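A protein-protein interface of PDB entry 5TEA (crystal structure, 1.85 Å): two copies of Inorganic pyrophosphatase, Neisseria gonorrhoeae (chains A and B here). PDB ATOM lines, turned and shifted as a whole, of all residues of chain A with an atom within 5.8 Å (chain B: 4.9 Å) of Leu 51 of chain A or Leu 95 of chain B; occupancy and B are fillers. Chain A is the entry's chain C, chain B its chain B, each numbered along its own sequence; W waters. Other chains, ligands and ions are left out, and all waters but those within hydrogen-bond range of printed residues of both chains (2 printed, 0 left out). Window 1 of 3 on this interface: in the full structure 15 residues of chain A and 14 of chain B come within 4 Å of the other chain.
The backbone carbonyl oxygen of Phe 49 of chain A sits close to the backbone NH of Phe 94 of chain B (3.2 Å). The backbone carbonyl oxygen (O) of Phe 94 of chain B lies within hydrogen-bond range of the backbone NH (N) of Leu 51 of chain A (2.8 Å).
The backbone carbonyl oxygen (O) of Val 28 of chain B lies within hydrogen-bond range of the backbone NH (N) of Leu 95 of chain B, at 2.9 Å. N of Gln 50 of chain A sits at hydrogen-bond distance from O of Glu 41 of chain A, 2.9 Å away.
Among the printed residues, pairs that only touch across the chains: His 38 of chain A with Leu 89 of chain B (3.4 Å), Phe 49 of chain A with Val 93 of chain B (3.6 Å), Gln 50 of chain A with Phe 94 of chain B (3.3 Å), Leu 51 of chain A with Leu 89 of chain B (3.7 Å), Leu 51 of chain A with Leu 95 of chain B (3.5 Å) and Ile 54 of chain A with Pro 119 of chain B (3.8 Å).
Printed residues of chain B within 4 Å of Leu 51 of chain A: Leu 89, Phe 94 and Leu 95. Of chain A, only Leu 51 comes within 4 Å of Leu 95 of chain B. Of the printed residues of chain A, Pro 119 of chain B touches Ile 54 (3.8 Å). Of the printed residues of chain B, Gln 50 of chain A touches Phe 94 (3.3 Å). Of the printed residues of chain B, Ile 54 of chain A touches Pro 119 (3.8 Å). Of the printed residues of chain B, Phe 49 of chain A touches Val 93 and Phe 94. Lys 39 of chain A touches none of the printed residues of chain B. The nearest residue of chain A that does not touch Leu 95 of chain B is Gln 50 of chain A (4.6 Å).
Of the 10 printed residues of chain A, 5 touch a printed residue of chain B. Printed residues of chain A that touch a printed residue of chain B: His 38, Phe 49, Gln 50, Leu 51 and Ile 54. Hydrophobic or aromatic side chains of chain A within 4 Å of the printed part of chain B: His 38, Leu 51 and Ile 54. Of the 11 printed residues of chain B, 5 touch a printed residue of chain A. Printed residues of chain B that touch a printed residue of chain A: Leu 89, Val 93, Phe 94, Leu 95 and Pro 119. Among the printed residues, 8 pairs touch across the chains.
No position is printed for both chains. Of the 8 pairs that touch across the chains among the printed residues, none has its exchanged pair printed and touching as well.
Water W1 lies within hydrogen-bond range of the backbone carbonyl oxygen (O) of Leu 51 of chain A (2.7 Å), the backbone NH (N) of Glu 96 of chain B (2.9 Å), the side-chain amide nitrogen (NE2) of Gln 50 of chain A (3.0 Å) and the backbone carbonyl oxygen (O) of Asp 52 of chain A (3.5 Å). Water W2 bridges the backbone carbonyl oxygen (O) of Glu 96 of chain B and the backbone carbonyl oxygen (O) of Asp 52 of chain A.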
ATOM      1  N   HIS A  38      12.266  28.568  -5.459  1.00  0.00           N
ATOM      2  CA  HIS A  38      13.039  27.799  -6.422  1.00  0.00           C
ATOM      3  C   HIS A  38      14.135  28.692  -6.988  1.00  0.00           C
ATOM      4  O   HIS A  38      13.837  29.749  -7.550  1.00  0.00           O
ATOM      5  CB  HIS A  38      12.122  27.270  -7.524  1.00  0.00           C
ATOM      6  CG  HIS A  38      11.087  26.317  -7.026  1.00  0.00           C
ATOM      7  ND1 HIS A  38      10.055  25.852  -7.814  1.00  0.00           N
ATOM      8  CD2 HIS A  38      10.928  25.735  -5.814  1.00  0.00           C
ATOM      9  CE1 HIS A  38       9.307  25.022  -7.108  1.00  0.00           C
ATOM     10  NE2 HIS A  38       9.808  24.943  -5.888  1.00  0.00           N
ATOM     11  N   LYS A  39      15.404  28.307  -6.793  1.00  0.00           N
ATOM     12  CA  LYS A  39      16.510  29.112  -7.315  1.00  0.00           C
ATOM     13  C   LYS A  39      16.741  28.680  -8.760  1.00  0.00           C
ATOM     14  O   LYS A  39      17.343  27.636  -9.032  1.00  0.00           O
ATOM     15  CB  LYS A  39      17.773  28.979  -6.467  1.00  0.00           C
ATOM     16  CG  LYS A  39      18.898  29.900  -6.933  1.00  0.00           C
ATOM     17  CD  LYS A  39      20.219  29.665  -6.170  1.00  0.00           C
ATOM     18  CE  LYS A  39      21.289  30.673  -6.572  1.00  0.00           C
ATOM     19  NZ  LYS A  39      21.708  30.554  -7.997  1.00  0.00           N
ATOM     20  N   ILE A  40      16.231  29.478  -9.685  1.00  0.00           N
ATOM     21  CA  ILE A  40      16.352  29.235 -11.112  1.00  0.00           C
ATOM     22  C   ILE A  40      17.352  30.229 -11.686  1.00  0.00           C
ATOM     23  O   ILE A  40      17.334  31.419 -11.338  1.00  0.00           O
ATOM     24  CB  ILE A  40      14.982  29.351 -11.809  1.00  0.00           C
ATOM     25  CG1 ILE A  40      13.997  28.353 -11.194  1.00  0.00           C
ATOM     26  CG2 ILE A  40      15.127  29.103 -13.299  1.00  0.00           C
ATOM     27  CD1 ILE A  40      12.546  28.594 -11.595  1.00  0.00           C
ATOM     28  N   GLU A  41      18.215  29.741 -12.574  1.00  0.00           N
ATOM     29  CA  GLU A  41      19.248  30.572 -13.168  1.00  0.00           C
ATOM     30  C   GLU A  41      19.336  30.253 -14.650  1.00  0.00           C
ATOM     31  O   GLU A  41      19.237  29.094 -15.044  1.00  0.00           O
ATOM     32  CB  GLU A  41      20.576  30.317 -12.459  1.00  0.00           C
ATOM     33  CG  GLU A  41      21.818  30.799 -13.138  1.00  0.00           C
ATOM     34  CD  GLU A  41      23.053  30.323 -12.396  1.00  0.00           C
ATOM     35  OE1 GLU A  41      23.138  29.108 -12.110  1.00  0.00           O
ATOM     36  OE2 GLU A  41      23.918  31.163 -12.073  1.00  0.00           O
ATOM     37  N   PHE A  49      17.088  27.348 -18.735  1.00  0.00           N
ATOM     38  CA  PHE A  49      16.908  27.712 -17.337  1.00  0.00           C
ATOM     39  C   PHE A  49      17.066  26.481 -16.450  1.00  0.00           C
ATOM     40  O   PHE A  49      16.460  25.437 -16.712  1.00  0.00           O
ATOM     41  CB  PHE A  49      15.544  28.373 -17.127  1.00  0.00           C
ATOM     42  CG  PHE A  49      15.446  29.741 -17.745  1.00  0.00           C
ATOM     43  CD1 PHE A  49      15.920  30.855 -17.066  1.00  0.00           C
ATOM     44  CD2 PHE A  49      14.892  29.908 -19.008  1.00  0.00           C
ATOM     45  CE1 PHE A  49      15.835  32.130 -17.633  1.00  0.00           C
ATOM     46  CE2 PHE A  49      14.810  31.174 -19.592  1.00  0.00           C
ATOM     47  CZ  PHE A  49      15.277  32.286 -18.901  1.00  0.00           C
ATOM     48  N   GLN A  50      17.900  26.600 -15.415  1.00  0.00           N
ATOM     49  CA  GLN A  50      18.227  25.486 -14.532  1.00  0.00           C
ATOM     50  C   GLN A  50      17.735  25.796 -13.127  1.00  0.00           C
ATOM     51  O   GLN A  50      17.979  26.891 -12.611  1.00  0.00           O
ATOM     52  CB  GLN A  50      19.741  25.210 -14.504  1.00  0.00           C
ATOM     53  CG  GLN A  50      20.157  24.134 -13.490  1.00  0.00           C
ATOM     54  CD  GLN A  50      21.641  23.811 -13.551  1.00  0.00           C
ATOM     55  OE1 GLN A  50      22.388  24.417 -14.312  1.00  0.00           O
ATOM     56  NE2 GLN A  50      22.066  22.835 -12.761  1.00  0.00           N
ATOM     57  N   LEU A  51      17.036  24.840 -12.523  1.00  0.00           N
ATOM     58  CA  LEU A  51      16.715  24.893 -11.100  1.00  0.00           C
ATOM     59  C   LEU A  51      17.961  24.462 -10.350  1.00  0.00           C
ATOM     60  O   LEU A  51      18.285  23.270 -10.308  1.00  0.00           O
ATOM     61  CB  LEU A  51      15.545  23.981 -10.778  1.00  0.00           C
ATOM     62  CG  LEU A  51      15.274  23.785  -9.293  1.00  0.00           C
ATOM     63  CD1 LEU A  51      14.747  25.059  -8.699  1.00  0.00           C
ATOM     64  CD2 LEU A  51      14.286  22.654  -9.088  1.00  0.00           C
ATOM     65  N   ASP A  52      18.689  25.432  -9.791  1.00  0.00           N
ATOM     66  CA  ASP A  52      19.915  25.098  -9.067  1.00  0.00           C
ATOM     67  C   ASP A  52      19.605  24.337  -7.785  1.00  0.00           C
ATOM     68  O   ASP A  52      20.302  23.374  -7.443  1.00  0.00           O
ATOM     69  CB  ASP A  52      20.708  26.361  -8.719  1.00  0.00           C
ATOM     70  CG  ASP A  52      21.365  27.011  -9.921  1.00  0.00           C
ATOM     71  OD1 ASP A  52      21.607  26.335 -10.949  1.00  0.00           O
ATOM     72  OD2 ASP A  52      21.659  28.219  -9.815  1.00  0.00           O
ATOM     73  N   ARG A  53      18.576  24.768  -7.054  1.00  0.00           N
ATOM     74  CA  ARG A  53      18.294  24.217  -5.735  1.00  0.00           C
ATOM     75  C   ARG A  53      16.950  24.733  -5.245  1.00  0.00           C
ATOM     76  O   ARG A  53      16.431  25.728  -5.744  1.00  0.00           O
ATOM     77  CB  ARG A  53      19.393  24.593  -4.736  1.00  0.00           C
ATOM     78  CG  ARG A  53      19.483  26.099  -4.419  1.00  0.00           C
ATOM     79  CD  ARG A  53      20.435  26.254  -3.252  1.00  0.00           C
ATOM     80  NE  ARG A  53      20.623  27.628  -2.796  1.00  0.00           N
ATOM     81  CZ  ARG A  53      21.663  28.390  -3.123  1.00  0.00           C
ATOM     82  NH1 ARG A  53      22.606  27.912  -3.930  1.00  0.00           N
ATOM     83  NH2 ARG A  53      21.763  29.627  -2.635  1.00  0.00           N
ATOM     84  N   ILE A  54      16.407  24.050  -4.249  1.00  0.00           N
ATOM     85  CA  ILE A  54      15.255  24.542  -3.500  1.00  0.00           C
ATOM     86  C   ILE A  54      15.781  25.324  -2.309  1.00  0.00           C
ATOM     87  O   ILE A  54      16.645  24.832  -1.575  1.00  0.00           O
ATOM     88  CB  ILE A  54      14.367  23.382  -3.015  1.00  0.00           C
ATOM     89  CG1 ILE A  54      14.053  22.406  -4.157  1.00  0.00           C
ATOM     90  CG2 ILE A  54      13.122  23.945  -2.299  1.00  0.00           C
ATOM     91  CD1 ILE A  54      13.145  22.966  -5.264  1.00  0.00           C
ATOM     92  N   ILE B  26      21.290  12.726 -11.410  1.00  0.00           N
ATOM     93  CA  ILE B  26      21.042  12.744 -12.846  1.00  0.00           C
ATOM     94  C   ILE B  26      20.421  14.080 -13.244  1.00  0.00           C
ATOM     95  O   ILE B  26      19.982  14.861 -12.401  1.00  0.00           O
ATOM     96  CB  ILE B  26      20.130  11.590 -13.281  1.00  0.00           C
ATOM     97  CG1 ILE B  26      18.738  11.778 -12.657  1.00  0.00           C
ATOM     98  CG2 ILE B  26      20.791  10.245 -12.927  1.00  0.00           C
ATOM     99  CD1 ILE B  26      17.736  10.730 -13.056  1.00  0.00           C
ATOM    100  N   ASN B  27      20.337  14.308 -14.559  1.00  0.00           N
ATOM    101  CA  ASN B  27      19.686  15.502 -15.089  1.00  0.00           C
ATOM    102  C   ASN B  27      18.244  15.164 -15.440  1.00  0.00           C
ATOM    103  O   ASN B  27      17.980  14.137 -16.074  1.00  0.00           O
ATOM    104  CB  ASN B  27      20.432  16.040 -16.318  1.00  0.00           C
ATOM    105  CG  ASN B  27      21.838  16.517 -15.984  1.00  0.00           C
ATOM    106  OD1 ASN B  27      22.067  17.081 -14.921  1.00  0.00           O
ATOM    107  ND2 ASN B  27      22.785  16.272 -16.880  1.00  0.00           N
ATOM    108  N   VAL B  28      17.318  16.027 -15.026  1.00  0.00           N
ATOM    109  CA  VAL B  28      15.887  15.834 -15.246  1.00  0.00           C
ATOM    110  C   VAL B  28      15.320  17.111 -15.843  1.00  0.00           C
ATOM    111  O   VAL B  28      15.675  18.214 -15.416  1.00  0.00           O
ATOM    112  CB  VAL B  28      15.161  15.468 -13.927  1.00  0.00           C
ATOM    113  CG1 VAL B  28      13.645  15.517 -14.100  1.00  0.00           C
ATOM    114  CG2 VAL B  28      15.595  14.069 -13.497  1.00  0.00           C
ATOM    115  N   LEU B  83       9.165  13.571  -9.934  1.00  0.00           N
ATOM    116  CA  LEU B  83      10.016  14.461  -9.155  1.00  0.00           C
ATOM    117  C   LEU B  83       9.190  15.044  -8.021  1.00  0.00           C
ATOM    118  O   LEU B  83       8.224  15.780  -8.267  1.00  0.00           O
ATOM    119  CB  LEU B  83      10.588  15.572 -10.032  1.00  0.00           C
ATOM    120  CG  LEU B  83      11.459  16.599  -9.296  1.00  0.00           C
ATOM    121  CD1 LEU B  83      12.818  15.983  -8.965  1.00  0.00           C
ATOM    122  CD2 LEU B  83      11.609  17.863 -10.134  1.00  0.00           C
ATOM    123  N   LEU B  89       6.940  22.540  -9.535  1.00  0.00           N
ATOM    124  CA  LEU B  89       7.936  23.076 -10.449  1.00  0.00           C
ATOM    125  C   LEU B  89       7.314  23.415 -11.802  1.00  0.00           C
ATOM    126  O   LEU B  89       6.451  22.688 -12.296  1.00  0.00           O
ATOM    127  CB  LEU B  89       9.061  22.046 -10.612  1.00  0.00           C
ATOM    128  CG  LEU B  89      10.420  22.505 -11.113  1.00  0.00           C
ATOM    129  CD1 LEU B  89      10.947  23.625 -10.236  1.00  0.00           C
ATOM    130  CD2 LEU B  89      11.403  21.322 -11.165  1.00  0.00           C
ATOM    131  N   VAL B  93      11.968  23.819 -16.930  1.00  0.00           N
ATOM    132  CA  VAL B  93      13.240  23.956 -16.226  1.00  0.00           C
ATOM    133  C   VAL B  93      13.855  22.575 -16.063  1.00  0.00           C
ATOM    134  O   VAL B  93      13.157  21.565 -15.943  1.00  0.00           O
ATOM    135  CB  VAL B  93      13.084  24.656 -14.856  1.00  0.00           C
ATOM    136  CG1 VAL B  93      12.404  26.015 -15.008  1.00  0.00           C
ATOM    137  CG2 VAL B  93      12.339  23.771 -13.874  1.00  0.00           C
ATOM    138  N   PHE B  94      15.183  22.520 -16.087  1.00  0.00           N
ATOM    139  CA  PHE B  94      15.888  21.279 -15.815  1.00  0.00           C
ATOM    140  C   PHE B  94      16.663  21.428 -14.514  1.00  0.00           C
ATOM    141  O   PHE B  94      16.902  22.540 -14.039  1.00  0.00           O
ATOM    142  CB  PHE B  94      16.819  20.892 -16.967  1.00  0.00           C
ATOM    143  CG  PHE B  94      18.126  21.647 -16.984  1.00  0.00           C
ATOM    144  CD1 PHE B  94      18.221  22.883 -17.610  1.00  0.00           C
ATOM    145  CD2 PHE B  94      19.255  21.119 -16.385  1.00  0.00           C
ATOM    146  CE1 PHE B  94      19.422  23.582 -17.630  1.00  0.00           C
ATOM    147  CE2 PHE B  94      20.460  21.825 -16.392  1.00  0.00           C
ATOM    148  CZ  PHE B  94      20.539  23.044 -17.024  1.00  0.00           C
ATOM    149  N   LEU B  95      17.038  20.291 -13.928  1.00  0.00           N
ATOM    150  CA  LEU B  95      17.716  20.296 -12.636  1.00  0.00           C
ATOM    151  C   LEU B  95      18.546  19.030 -12.477  1.00  0.00           C
ATOM    152  O   LEU B  95      18.273  17.997 -13.094  1.00  0.00           O
ATOM    153  CB  LEU B  95      16.721  20.398 -11.478  1.00  0.00           C
ATOM    154  CG  LEU B  95      15.877  19.139 -11.182  1.00  0.00           C
ATOM    155  CD1 LEU B  95      15.383  19.188  -9.742  1.00  0.00           C
ATOM    156  CD2 LEU B  95      14.685  19.033 -12.133  1.00  0.00           C
ATOM    157  N   GLU B  96      19.554  19.125 -11.621  1.00  0.00           N
ATOM    158  CA  GLU B  96      20.213  17.943 -11.096  1.00  0.00           C
ATOM    159  C   GLU B  96      19.342  17.362  -9.995  1.00  0.00           C
ATOM    160  O   GLU B  96      18.908  18.082  -9.084  1.00  0.00           O
ATOM    161  CB  GLU B  96      21.605  18.304 -10.567  1.00  0.00           C
ATOM    162  CG  GLU B  96      22.491  18.831 -11.677  1.00  0.00           C
ATOM    163  CD  GLU B  96      23.944  19.001 -11.254  1.00  0.00           C
ATOM    164  OE1 GLU B  96      24.257  18.693 -10.088  1.00  0.00           O
ATOM    165  OE2 GLU B  96      24.760  19.448 -12.088  1.00  0.00           O
ATOM    166  N   ALA B  97      19.068  16.063 -10.086  1.00  0.00           N
ATOM    167  CA  ALA B  97      18.132  15.414  -9.181  1.00  0.00           C
ATOM    168  C   ALA B  97      18.733  14.131  -8.634  1.00  0.00           C
ATOM    169  O   ALA B  97      19.443  13.417  -9.345  1.00  0.00           O
ATOM    170  CB  ALA B  97      16.806  15.106  -9.884  1.00  0.00           C
ATOM    171  N   PRO B 119      14.981  16.934  -5.967  1.00  0.00           N
ATOM    172  CA  PRO B 119      16.090  17.836  -6.309  1.00  0.00           C
ATOM    173  C   PRO B 119      17.330  17.458  -5.513  1.00  0.00           C
ATOM    174  O   PRO B 119      17.243  17.090  -4.335  1.00  0.00           O
ATOM    175  CB  PRO B 119      15.567  19.220  -5.903  1.00  0.00           C
ATOM    176  CG  PRO B 119      14.061  19.070  -5.902  1.00  0.00           C
ATOM    177  CD  PRO B 119      13.833  17.669  -5.403  1.00  0.00           C
HETATM  178  O   HOH W   1      20.424  21.685 -10.494  1.00  0.00           O
HETATM  179  O   HOH W   2      19.167  20.368  -7.269  1.00  0.00           O
